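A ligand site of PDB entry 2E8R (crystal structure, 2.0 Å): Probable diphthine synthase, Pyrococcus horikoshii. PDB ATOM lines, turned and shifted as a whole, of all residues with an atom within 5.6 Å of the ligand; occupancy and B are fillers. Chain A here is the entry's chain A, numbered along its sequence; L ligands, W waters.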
ATOM      1  N   LEU A  10     -11.383  10.751   0.912  1.00  0.00           N
ATOM      2  CA  LEU A  10     -12.571  11.519   0.489  1.00  0.00           C
ATOM      3  C   LEU A  10     -12.485  13.063   0.297  1.00  0.00           C
ATOM      4  O   LEU A  10     -13.053  13.572  -0.643  1.00  0.00           O
ATOM      5  CB  LEU A  10     -13.687  11.256   1.469  1.00  0.00           C
ATOM      6  CG  LEU A  10     -14.098   9.813   1.632  1.00  0.00           C
ATOM      7  CD1 LEU A  10     -14.906   9.658   2.945  1.00  0.00           C
ATOM      8  CD2 LEU A  10     -14.991   9.358   0.467  1.00  0.00           C
ATOM      9  N   TYR A  11     -11.869  13.780   1.271  1.00  0.00           N
ATOM     10  CA  TYR A  11     -11.996  15.256   1.230  1.00  0.00           C
ATOM     11  C   TYR A  11     -10.667  16.061   1.313  1.00  0.00           C
ATOM     12  O   TYR A  11     -10.475  16.993   0.538  1.00  0.00           O
ATOM     13  CB  TYR A  11     -12.937  15.648   2.356  1.00  0.00           C
ATOM     14  CG  TYR A  11     -13.229  17.141   2.414  1.00  0.00           C
ATOM     15  CD1 TYR A  11     -14.068  17.746   1.474  1.00  0.00           C
ATOM     16  CD2 TYR A  11     -12.728  17.910   3.471  1.00  0.00           C
ATOM     17  CE1 TYR A  11     -14.384  19.099   1.583  1.00  0.00           C
ATOM     18  CE2 TYR A  11     -13.043  19.254   3.570  1.00  0.00           C
ATOM     19  CZ  TYR A  11     -13.848  19.865   2.639  1.00  0.00           C
ATOM     20  OH  TYR A  11     -14.147  21.200   2.728  1.00  0.00           O
ATOM     21  N   THR A  36     -10.129  11.454 -11.543  1.00  0.00           N
ATOM     22  CA  THR A  36     -11.157  10.463 -11.237  1.00  0.00           C
ATOM     23  C   THR A  36     -12.111  10.942 -10.148  1.00  0.00           C
ATOM     24  O   THR A  36     -13.204  10.388  -9.983  1.00  0.00           O
ATOM     25  CB  THR A  36     -10.558   9.110 -10.801  1.00  0.00           C
ATOM     26  OG1 THR A  36      -9.708   9.295  -9.661  1.00  0.00           O
ATOM     27  CG2 THR A  36      -9.777   8.491 -11.927  1.00  0.00           C
ATOM     28  N   SER A  37     -11.698  11.959  -9.408  1.00  0.00           N
ATOM     29  CA  SER A  37     -12.550  12.485  -8.350  1.00  0.00           C
ATOM     30  C   SER A  37     -12.058  13.842  -7.915  1.00  0.00           C
ATOM     31  O   SER A  37     -11.049  14.341  -8.397  1.00  0.00           O
ATOM     32  CB  SER A  37     -12.581  11.528  -7.161  1.00  0.00           C
ATOM     33  OG  SER A  37     -13.561  11.926  -6.231  1.00  0.00           O
ATOM     34  N   LEU A  38     -12.780  14.444  -6.974  1.00  0.00           N
ATOM     35  CA  LEU A  38     -12.415  15.755  -6.464  1.00  0.00           C
ATOM     36  C   LEU A  38     -12.277  15.749  -4.954  1.00  0.00           C
ATOM     37  O   LEU A  38     -13.174  15.310  -4.239  1.00  0.00           O
ATOM     38  CB  LEU A  38     -13.459  16.798  -6.877  1.00  0.00           C
ATOM     39  CG  LEU A  38     -13.344  18.205  -6.290  1.00  0.00           C
ATOM     40  CD1 LEU A  38     -12.078  18.890  -6.812  1.00  0.00           C
ATOM     41  CD2 LEU A  38     -14.587  19.014  -6.652  1.00  0.00           C
ATOM     42  N   PRO A  85      -7.463  10.140  -5.587  1.00  0.00           N
ATOM     43  CA  PRO A  85      -8.456  10.565  -4.597  1.00  0.00           C
ATOM     44  C   PRO A  85      -9.206   9.300  -4.174  1.00  0.00           C
ATOM     45  O   PRO A  85      -9.222   8.310  -4.914  1.00  0.00           O
ATOM     46  CB  PRO A  85      -9.364  11.516  -5.384  1.00  0.00           C
ATOM     47  CG  PRO A  85      -8.462  12.025  -6.478  1.00  0.00           C
ATOM     48  CD  PRO A  85      -7.709  10.786  -6.883  1.00  0.00           C
ATOM     49  N   GLY A  86      -9.820   9.322  -2.993  1.00  0.00           N
ATOM     50  CA  GLY A  86     -10.563   8.169  -2.516  1.00  0.00           C
ATOM     51  C   GLY A  86      -9.762   6.888  -2.506  1.00  0.00           C
ATOM     52  O   GLY A  86      -8.599   6.889  -2.111  1.00  0.00           O
ATOM     53  N   ASP A  87     -10.396   5.774  -2.914  1.00  0.00           N
ATOM     54  CA  ASP A  87      -9.714   4.483  -3.000  1.00  0.00           C
ATOM     55  C   ASP A  87      -9.307   4.354  -4.459  1.00  0.00           C
ATOM     56  O   ASP A  87     -10.128   4.528  -5.362  1.00  0.00           O
ATOM     57  CB  ASP A  87     -10.641   3.341  -2.600  1.00  0.00           C
ATOM     58  CG  ASP A  87      -9.952   1.982  -2.674  1.00  0.00           C
ATOM     59  OD1 ASP A  87      -9.628   1.548  -3.802  1.00  0.00           O
ATOM     60  OD2 ASP A  87      -9.735   1.351  -1.609  1.00  0.00           O
ATOM     61  N   PRO A  88      -8.035   4.039  -4.717  1.00  0.00           N
ATOM     62  CA  PRO A  88      -7.488   3.885  -6.072  1.00  0.00           C
ATOM     63  C   PRO A  88      -8.193   2.957  -7.052  1.00  0.00           C
ATOM     64  O   PRO A  88      -8.105   3.166  -8.263  1.00  0.00           O
ATOM     65  CB  PRO A  88      -6.036   3.465  -5.808  1.00  0.00           C
ATOM     66  CG  PRO A  88      -6.129   2.719  -4.517  1.00  0.00           C
ATOM     67  CD  PRO A  88      -7.049   3.589  -3.708  1.00  0.00           C
ATOM     68  N   LEU A  89      -8.890   1.942  -6.549  1.00  0.00           N
ATOM     69  CA  LEU A  89      -9.545   0.990  -7.446  1.00  0.00           C
ATOM     70  C   LEU A  89     -11.058   1.053  -7.530  1.00  0.00           C
ATOM     71  O   LEU A  89     -11.675   0.267  -8.247  1.00  0.00           O
ATOM     72  CB  LEU A  89      -9.140  -0.433  -7.046  1.00  0.00           C
ATOM     73  CG  LEU A  89      -7.638  -0.638  -6.821  1.00  0.00           C
ATOM     74  CD1 LEU A  89      -7.386  -2.101  -6.524  1.00  0.00           C
ATOM     75  CD2 LEU A  89      -6.863  -0.201  -8.054  1.00  0.00           C
ATOM     76  N   VAL A  90     -11.659   1.985  -6.796  1.00  0.00           N
ATOM     77  CA  VAL A  90     -13.119   2.103  -6.781  1.00  0.00           C
ATOM     78  C   VAL A  90     -13.639   3.067  -7.848  1.00  0.00           C
ATOM     79  O   VAL A  90     -13.326   4.248  -7.832  1.00  0.00           O
ATOM     80  CB  VAL A  90     -13.609   2.561  -5.391  1.00  0.00           C
ATOM     81  CG1 VAL A  90     -15.116   2.850  -5.426  1.00  0.00           C
ATOM     82  CG2 VAL A  90     -13.296   1.475  -4.373  1.00  0.00           C
ATOM     83  N   ALA A  91     -14.448   2.543  -8.765  1.00  0.00           N
ATOM     84  CA  ALA A  91     -15.045   3.348  -9.824  1.00  0.00           C
ATOM     85  C   ALA A  91     -13.989   4.048 -10.683  1.00  0.00           C
ATOM     86  O   ALA A  91     -14.163   5.194 -11.082  1.00  0.00           O
ATOM     87  CB  ALA A  91     -16.018   4.378  -9.233  1.00  0.00           C
ATOM     88  N   THR A  92     -12.884   3.357 -10.915  1.00  0.00           N
ATOM     89  CA  THR A  92     -11.836   3.792 -11.807  1.00  0.00           C
ATOM     90  C   THR A  92     -11.407   2.589 -12.625  1.00  0.00           C
ATOM     91  O   THR A  92     -11.836   1.475 -12.402  1.00  0.00           O
ATOM     92  CB  THR A  92     -10.641   4.321 -10.994  1.00  0.00           C
ATOM     93  OG1 THR A  92      -9.934   3.240 -10.388  1.00  0.00           O
ATOM     94  CG2 THR A  92     -11.099   5.300  -9.901  1.00  0.00           C
ATOM     95  N   PRO A 114     -10.450   5.860   2.659  1.00  0.00           N
ATOM     96  CA  PRO A 114     -11.906   5.951   2.642  1.00  0.00           C
ATOM     97  C   PRO A 114     -12.434   6.255   1.235  1.00  0.00           C
ATOM     98  O   PRO A 114     -11.883   7.083   0.503  1.00  0.00           O
ATOM     99  CB  PRO A 114     -12.217   7.048   3.667  1.00  0.00           C
ATOM    100  CG  PRO A 114     -10.910   7.795   3.836  1.00  0.00           C
ATOM    101  CD  PRO A 114      -9.864   6.727   3.698  1.00  0.00           C
ATOM    102  N   SER A 115     -13.505   5.560   0.869  1.00  0.00           N
ATOM    103  CA  SER A 115     -14.123   5.684  -0.448  1.00  0.00           C
ATOM    104  C   SER A 115     -15.573   6.173  -0.368  1.00  0.00           C
ATOM    105  O   SER A 115     -16.264   5.907   0.623  1.00  0.00           O
ATOM    106  CB  SER A 115     -14.108   4.322  -1.144  1.00  0.00           C
ATOM    107  OG  SER A 115     -14.887   4.329  -2.330  1.00  0.00           O
ATOM    108  N   ILE A 116     -16.029   6.875  -1.398  1.00  0.00           N
ATOM    109  CA  ILE A 116     -17.406   7.361  -1.411  1.00  0.00           C
ATOM    110  C   ILE A 116     -18.349   6.155  -1.379  1.00  0.00           C
ATOM    111  O   ILE A 116     -19.438   6.225  -0.824  1.00  0.00           O
ATOM    112  CB  ILE A 116     -17.722   8.209  -2.674  1.00  0.00           C
ATOM    113  CG1 ILE A 116     -19.146   8.774  -2.582  1.00  0.00           C
ATOM    114  CG2 ILE A 116     -17.613   7.355  -3.940  1.00  0.00           C
ATOM    115  CD1 ILE A 116     -19.363   9.710  -1.399  1.00  0.00           C
ATOM    116  N   TYR A 117     -17.902   5.034  -1.946  1.00  0.00           N
ATOM    117  CA  TYR A 117     -18.723   3.837  -2.003  1.00  0.00           C
ATOM    118  C   TYR A 117     -19.177   3.339  -0.618  1.00  0.00           C
ATOM    119  O   TYR A 117     -20.289   2.820  -0.475  1.00  0.00           O
ATOM    120  CB  TYR A 117     -17.990   2.717  -2.748  1.00  0.00           C
ATOM    121  CG  TYR A 117     -18.879   1.553  -3.140  1.00  0.00           C
ATOM    122  CD1 TYR A 117     -19.824   1.686  -4.162  1.00  0.00           C
ATOM    123  CD2 TYR A 117     -18.800   0.333  -2.481  1.00  0.00           C
ATOM    124  CE1 TYR A 117     -20.669   0.621  -4.513  1.00  0.00           C
ATOM    125  CE2 TYR A 117     -19.625  -0.734  -2.818  1.00  0.00           C
ATOM    126  CZ  TYR A 117     -20.556  -0.584  -3.834  1.00  0.00           C
ATOM    127  OH  TYR A 117     -21.377  -1.645  -4.148  1.00  0.00           O
ATOM    128  N   LEU A 164     -25.578   6.650  -7.318  1.00  0.00           N
ATOM    129  CA  LEU A 164     -25.263   7.272  -8.600  1.00  0.00           C
ATOM    130  C   LEU A 164     -24.028   8.170  -8.523  1.00  0.00           C
ATOM    131  O   LEU A 164     -24.082   9.264  -7.974  1.00  0.00           O
ATOM    132  CB  LEU A 164     -26.445   8.098  -9.093  1.00  0.00           C
ATOM    133  CG  LEU A 164     -27.776   7.369  -9.317  1.00  0.00           C
ATOM    134  CD1 LEU A 164     -28.886   8.385  -9.553  1.00  0.00           C
ATOM    135  CD2 LEU A 164     -27.646   6.409 -10.489  1.00  0.00           C
ATOM    136  N   PHE A 165     -22.918   7.682  -9.071  1.00  0.00           N
ATOM    137  CA  PHE A 165     -21.689   8.465  -9.129  1.00  0.00           C
ATOM    138  C   PHE A 165     -22.035   9.577 -10.118  1.00  0.00           C
ATOM    139  O   PHE A 165     -22.782   9.342 -11.063  1.00  0.00           O
ATOM    140  CB  PHE A 165     -20.551   7.627  -9.700  1.00  0.00           C
ATOM    141  CG  PHE A 165     -20.078   6.537  -8.783  1.00  0.00           C
ATOM    142  CD1 PHE A 165     -19.214   6.816  -7.732  1.00  0.00           C
ATOM    143  CD2 PHE A 165     -20.517   5.225  -8.961  1.00  0.00           C
ATOM    144  CE1 PHE A 165     -18.772   5.806  -6.878  1.00  0.00           C
ATOM    145  CE2 PHE A 165     -20.082   4.202  -8.107  1.00  0.00           C
ATOM    146  CZ  PHE A 165     -19.203   4.497  -7.068  1.00  0.00           C
ATOM    147  N   LEU A 166     -21.506  10.775  -9.897  1.00  0.00           N
ATOM    148  CA  LEU A 166     -21.808  11.874 -10.822  1.00  0.00           C
ATOM    149  C   LEU A 166     -20.602  12.204 -11.701  1.00  0.00           C
ATOM    150  O   LEU A 166     -19.454  12.085 -11.279  1.00  0.00           O
ATOM    151  CB  LEU A 166     -22.269  13.102 -10.038  1.00  0.00           C
ATOM    152  CG  LEU A 166     -23.492  12.872  -9.135  1.00  0.00           C
ATOM    153  CD1 LEU A 166     -23.993  14.217  -8.635  1.00  0.00           C
ATOM    154  CD2 LEU A 166     -24.611  12.140  -9.887  1.00  0.00           C
ATOM    155  N   ASP A 167     -20.871  12.613 -12.936  1.00  0.00           N
ATOM    156  CA  ASP A 167     -19.821  12.905 -13.902  1.00  0.00           C
ATOM    157  C   ASP A 167     -18.812  13.970 -13.478  1.00  0.00           C
ATOM    158  O   ASP A 167     -19.064  14.785 -12.577  1.00  0.00           O
ATOM    159  CB  ASP A 167     -20.464  13.311 -15.230  1.00  0.00           C
ATOM    160  CG  ASP A 167     -19.568  13.006 -16.427  1.00  0.00           C
ATOM    161  OD1 ASP A 167     -18.456  12.468 -16.219  1.00  0.00           O
ATOM    162  OD2 ASP A 167     -19.993  13.295 -17.567  1.00  0.00           O
ATOM    163  N   ILE A 168     -17.657  13.940 -14.135  1.00  0.00           N
ATOM    164  CA  ILE A 168     -16.604  14.901 -13.860  1.00  0.00           C
ATOM    165  C   ILE A 168     -15.706  15.114 -15.083  1.00  0.00           C
ATOM    166  O   ILE A 168     -15.296  14.156 -15.740  1.00  0.00           O
ATOM    167  CB  ILE A 168     -15.735  14.452 -12.658  1.00  0.00           C
ATOM    168  CG1 ILE A 168     -14.495  15.342 -12.544  1.00  0.00           C
ATOM    169  CG2 ILE A 168     -15.343  12.998 -12.803  1.00  0.00           C
ATOM    170  CD1 ILE A 168     -13.613  15.023 -11.359  1.00  0.00           C
ATOM    171  N   LEU A 206     -25.622  13.542  -0.959  1.00  0.00           N
ATOM    172  CA  LEU A 206     -24.486  13.580  -0.046  1.00  0.00           C
ATOM    173  C   LEU A 206     -23.403  14.394  -0.756  1.00  0.00           C
ATOM    174  O   LEU A 206     -22.969  14.029  -1.857  1.00  0.00           O
ATOM    175  CB  LEU A 206     -23.972  12.164   0.247  1.00  0.00           C
ATOM    176  CG  LEU A 206     -22.666  12.053   1.045  1.00  0.00           C
ATOM    177  CD1 LEU A 206     -22.779  12.798   2.367  1.00  0.00           C
ATOM    178  CD2 LEU A 206     -22.339  10.587   1.297  1.00  0.00           C
ATOM    179  N   ALA A 207     -22.995  15.489  -0.140  1.00  0.00           N
ATOM    180  CA  ALA A 207     -21.966  16.337  -0.736  1.00  0.00           C
ATOM    181  C   ALA A 207     -20.767  16.511   0.170  1.00  0.00           C
ATOM    182  O   ALA A 207     -20.910  16.756   1.368  1.00  0.00           O
ATOM    183  CB  ALA A 207     -22.554  17.720  -1.074  1.00  0.00           C
ATOM    184  N   ARG A 208     -19.589  16.405  -0.420  1.00  0.00           N
ATOM    185  CA  ARG A 208     -18.329  16.569   0.294  1.00  0.00           C
ATOM    186  C   ARG A 208     -18.197  15.618   1.487  1.00  0.00           C
ATOM    187  O   ARG A 208     -17.916  16.042   2.603  1.00  0.00           O
ATOM    188  CB  ARG A 208     -18.181  18.024   0.741  1.00  0.00           C
ATOM    189  CG  ARG A 208     -18.326  19.040  -0.406  1.00  0.00           C
ATOM    190  CD  ARG A 208     -18.253  20.484   0.098  1.00  0.00           C
ATOM    191  NE  ARG A 208     -19.176  20.702   1.208  1.00  0.00           N
ATOM    192  CZ  ARG A 208     -20.501  20.795   1.080  1.00  0.00           C
ATOM    193  NH1 ARG A 208     -21.064  20.706  -0.111  1.00  0.00           N
ATOM    194  NH2 ARG A 208     -21.249  20.946   2.155  1.00  0.00           N
ATOM    195  N   ALA A 209     -18.409  14.337   1.239  1.00  0.00           N
ATOM    196  CA  ALA A 209     -18.263  13.332   2.292  1.00  0.00           C
ATOM    197  C   ALA A 209     -16.788  13.425   2.678  1.00  0.00           C
ATOM    198  O   ALA A 209     -15.940  13.715   1.833  1.00  0.00           O
ATOM    199  CB  ALA A 209     -18.589  11.941   1.753  1.00  0.00           C
ATOM    200  N   GLY A 210     -16.467  13.183   3.943  1.00  0.00           N
ATOM    201  CA  GLY A 210     -15.088  13.275   4.367  1.00  0.00           C
ATOM    202  C   GLY A 210     -14.838  14.572   5.129  1.00  0.00           C
ATOM    203  O   GLY A 210     -13.944  14.654   5.968  1.00  0.00           O
ATOM    204  N   PRO A 233     -17.571  17.654  -4.491  1.00  0.00           N
ATOM    205  CA  PRO A 233     -18.356  16.699  -5.277  1.00  0.00           C
ATOM    206  C   PRO A 233     -19.648  16.255  -4.599  1.00  0.00           C
ATOM    207  O   PRO A 233     -19.783  16.358  -3.381  1.00  0.00           O
ATOM    208  CB  PRO A 233     -17.376  15.545  -5.460  1.00  0.00           C
ATOM    209  CG  PRO A 233     -16.653  15.532  -4.144  1.00  0.00           C
ATOM    210  CD  PRO A 233     -16.396  16.999  -3.875  1.00  0.00           C
ATOM    211  N   HIS A 234     -20.581  15.757  -5.403  1.00  0.00           N
ATOM    212  CA  HIS A 234     -21.868  15.277  -4.919  1.00  0.00           C
ATOM    213  C   HIS A 234     -22.135  13.893  -5.476  1.00  0.00           C
ATOM    214  O   HIS A 234     -21.593  13.510  -6.513  1.00  0.00           O
ATOM    215  CB  HIS A 234     -23.034  16.141  -5.442  1.00  0.00           C
ATOM    216  CG  HIS A 234     -22.992  17.580  -5.069  1.00  0.00           C
ATOM    217  ND1 HIS A 234     -23.947  18.476  -5.494  1.00  0.00           N
ATOM    218  CD2 HIS A 234     -22.131  18.289  -4.286  1.00  0.00           C
ATOM    219  CE1 HIS A 234     -23.693  19.670  -4.990  1.00  0.00           C
ATOM    220  NE2 HIS A 234     -22.595  19.584  -4.255  1.00  0.00           N
ATOM    221  N   ILE A 235     -22.984  13.150  -4.775  1.00  0.00           N
ATOM    222  CA  ILE A 235     -23.428  11.852  -5.275  1.00  0.00           C
ATOM    223  C   ILE A 235     -24.931  11.906  -5.078  1.00  0.00           C
ATOM    224  O   ILE A 235     -25.429  12.606  -4.190  1.00  0.00           O
ATOM    225  CB  ILE A 235     -22.891  10.631  -4.491  1.00  0.00           C
ATOM    226  CG1 ILE A 235     -23.250  10.726  -3.008  1.00  0.00           C
ATOM    227  CG2 ILE A 235     -21.400  10.503  -4.700  1.00  0.00           C
ATOM    228  CD1 ILE A 235     -22.993   9.450  -2.262  1.00  0.00           C
HETATM  229  N1  LIG L   1     -12.135   6.084  -6.357  1.00  0.00           N
HETATM  230  C1  LIG L   1     -13.141   7.120  -5.868  1.00  0.00           C
HETATM  231  C2  LIG L   1     -14.360   7.334  -6.708  1.00  0.00           C
HETATM  232  C3  LIG L   1     -14.175   7.738  -8.162  1.00  0.00           C
HETATM  233  S1  LIG L   1     -15.812   8.237  -8.823  1.00  0.00           S
HETATM  234  C4  LIG L   1     -13.534   6.689  -4.385  1.00  0.00           C
HETATM  235  O1  LIG L   1     -13.023   5.665  -3.896  1.00  0.00           O
HETATM  236  O2  LIG L   1     -14.371   7.456  -3.767  1.00  0.00           O
HETATM  237  C5  LIG L   1     -15.807   9.942  -8.403  1.00  0.00           C
HETATM  238  C6  LIG L   1     -17.288  10.416  -8.144  1.00  0.00           C
HETATM  239  O3  LIG L   1     -17.707   9.844  -6.888  1.00  0.00           O
HETATM  240  C7  LIG L   1     -17.457  11.898  -8.027  1.00  0.00           C
HETATM  241  O4  LIG L   1     -17.703  12.462  -9.310  1.00  0.00           O
HETATM  242  C8  LIG L   1     -18.636  11.988  -7.040  1.00  0.00           C
HETATM  243  O5  LIG L   1     -19.901  11.846  -7.699  1.00  0.00           O
HETATM  244  C9  LIG L   1     -18.330  10.883  -6.015  1.00  0.00           C
HETATM  245  N2  LIG L   1     -17.506  11.240  -4.999  1.00  0.00           N
HETATM  246  C10 LIG L   1     -16.166  11.031  -4.713  1.00  0.00           C
HETATM  247  N3  LIG L   1     -15.745  11.556  -3.593  1.00  0.00           N
HETATM  248  C11 LIG L   1     -16.906  12.186  -3.052  1.00  0.00           C
HETATM  249  C12 LIG L   1     -17.095  12.929  -1.830  1.00  0.00           C
HETATM  250  N4  LIG L   1     -16.137  13.173  -0.936  1.00  0.00           N
HETATM  251  N5  LIG L   1     -18.384  13.397  -1.640  1.00  0.00           N
HETATM  252  C13 LIG L   1     -19.399  13.186  -2.531  1.00  0.00           C
HETATM  253  N6  LIG L   1     -19.251  12.476  -3.702  1.00  0.00           N
HETATM  254  C14 LIG L   1     -17.976  12.007  -3.892  1.00  0.00           C
HETATM  255  O   HOH W   1     -12.535  12.383  -3.807  1.00  0.00           O
HETATM  256  O   HOH W   2     -18.072  15.227  -9.788  1.00  0.00           O
HETATM  257  O   HOH W   3     -10.578   8.145  -7.344  1.00  0.00           O
HETATM  258  O   HOH W   4     -13.334   9.993  -2.746  1.00  0.00           O
HETATM  259  O   HOH W   5     -14.228  15.960  -1.790  1.00  0.00           O
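An oxygen (O2) of the ligand sits at hydrogen-bond distance from the backbone NH of Ile 116, 2.9 Å away.
O of Val 90 sits at hydrogen-bond distance from N1 of the ligand, 2.6 Å away.
The side-chain hydroxyl (OG) of Ser 37 sits close to a nitrogen (N3) of the ligand (3.4 Å).
N of Leu 166 sits at hydrogen-bond distance from O5 of the ligand, at 2.9 Å.
N5 of the ligand is in hydrogen-bond range of N of Ala 209.
The backbone carbonyl oxygen (O) of Asp 87 is in hydrogen-bond range of a nitrogen (N1) of the ligand.
The backbone carbonyl oxygen (O) of Ala 209 lies within hydrogen-bond range of a nitrogen (N4) of the ligand (2.8 Å).
OG of Ser 115 is in hydrogen-bond range of O1 of the ligand (2.8 Å).
The backbone carbonyl oxygen (O) of Leu 166 lies within hydrogen-bond range of an oxygen (O4) of the ligand (2.7 Å).
A nitrogen (N4) of the ligand lies within hydrogen-bond range of the backbone carbonyl oxygen (O) of Leu 10, 3.1 Å away.
An oxygen (O5) of the ligand sits at hydrogen-bond distance from the backbone carbonyl oxygen of His 234, 2.7 Å away.
O1 of the ligand sits at hydrogen-bond distance from N of Asp 87, 2.8 Å away.
The backbone NH (N) of Arg 208 is in hydrogen-bond range of a nitrogen (N5) of the ligand (3.5 Å).
OD1 of Asp 87 lies within hydrogen-bond range of N of Leu 89, 2.9 Å away.
O of Leu 206 sits at hydrogen-bond distance from N of Ile 235 (3.0 Å).
The backbone carbonyl oxygen of Pro 233 sits at hydrogen-bond distance from the backbone NH of Arg 208 (3.0 Å).
The side-chain hydroxyl (OG) of Ser 115 sits close to the backbone NH (N) of Tyr 117, 3.1 Å away.
OG1 of Thr 92 sits at hydrogen-bond distance from O of Pro 88 (2.8 Å).
O of Thr 36 lies close to S1 of the ligand, 3.6 Å away.
Pro 85 touches the ligand (O to N1, 3.9 Å).
Gly 86 touches the ligand.
O of Ala 91 touches C3 of the ligand (3.9 Å).
CG2 of Thr 92 touches N1 of the ligand, at 3.8 Å.
CD1 of Phe 165 touches O3 of the ligand (3.5 Å).
O of Leu 206 touches C13 of the ligand, at 3.7 Å.
O of Pro 233 touches C13 of the ligand (3.3 Å).
Ile 235 touches the ligand.
Hydrophobic or aromatic side chains within 4 Å of the ligand: Leu 10, Val 90, Ala 91, Ile 116, Phe 165, Leu 166, Ala 209, Pro 233 and Ile 235.
Within 4 Å of the ligand: Leu 10, Thr 36, Ser 37, Pro 85, Gly 86, Asp 87, Val 90, Ala 91, Thr 92, Ser 115, Ile 116, Phe 165, Leu 166, Leu 206, Arg 208, Ala 209, Pro 233, His 234 and Ile 235.
The nearest printed residue that does not touch the ligand is Asp 167 (4.2 Å).
Water W3 lies within hydrogen-bond range of the side-chain hydroxyl (OG1) of Thr 36 (2.7 Å), a nitrogen (N1) of the ligand (2.8 Å) and the backbone carbonyl oxygen (O) of Pro 85 (2.8 Å).
Water W2 bridges an oxygen (O4) of the ligand (2.8 Å) and the backbone carbonyl oxygen of Asp 167 (3.0 Å).
Water W5 lies within hydrogen-bond range of O of Leu 38 (2.7 Å), O of Leu 10 (2.9 Å) and N4 of the ligand (3.5 Å).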
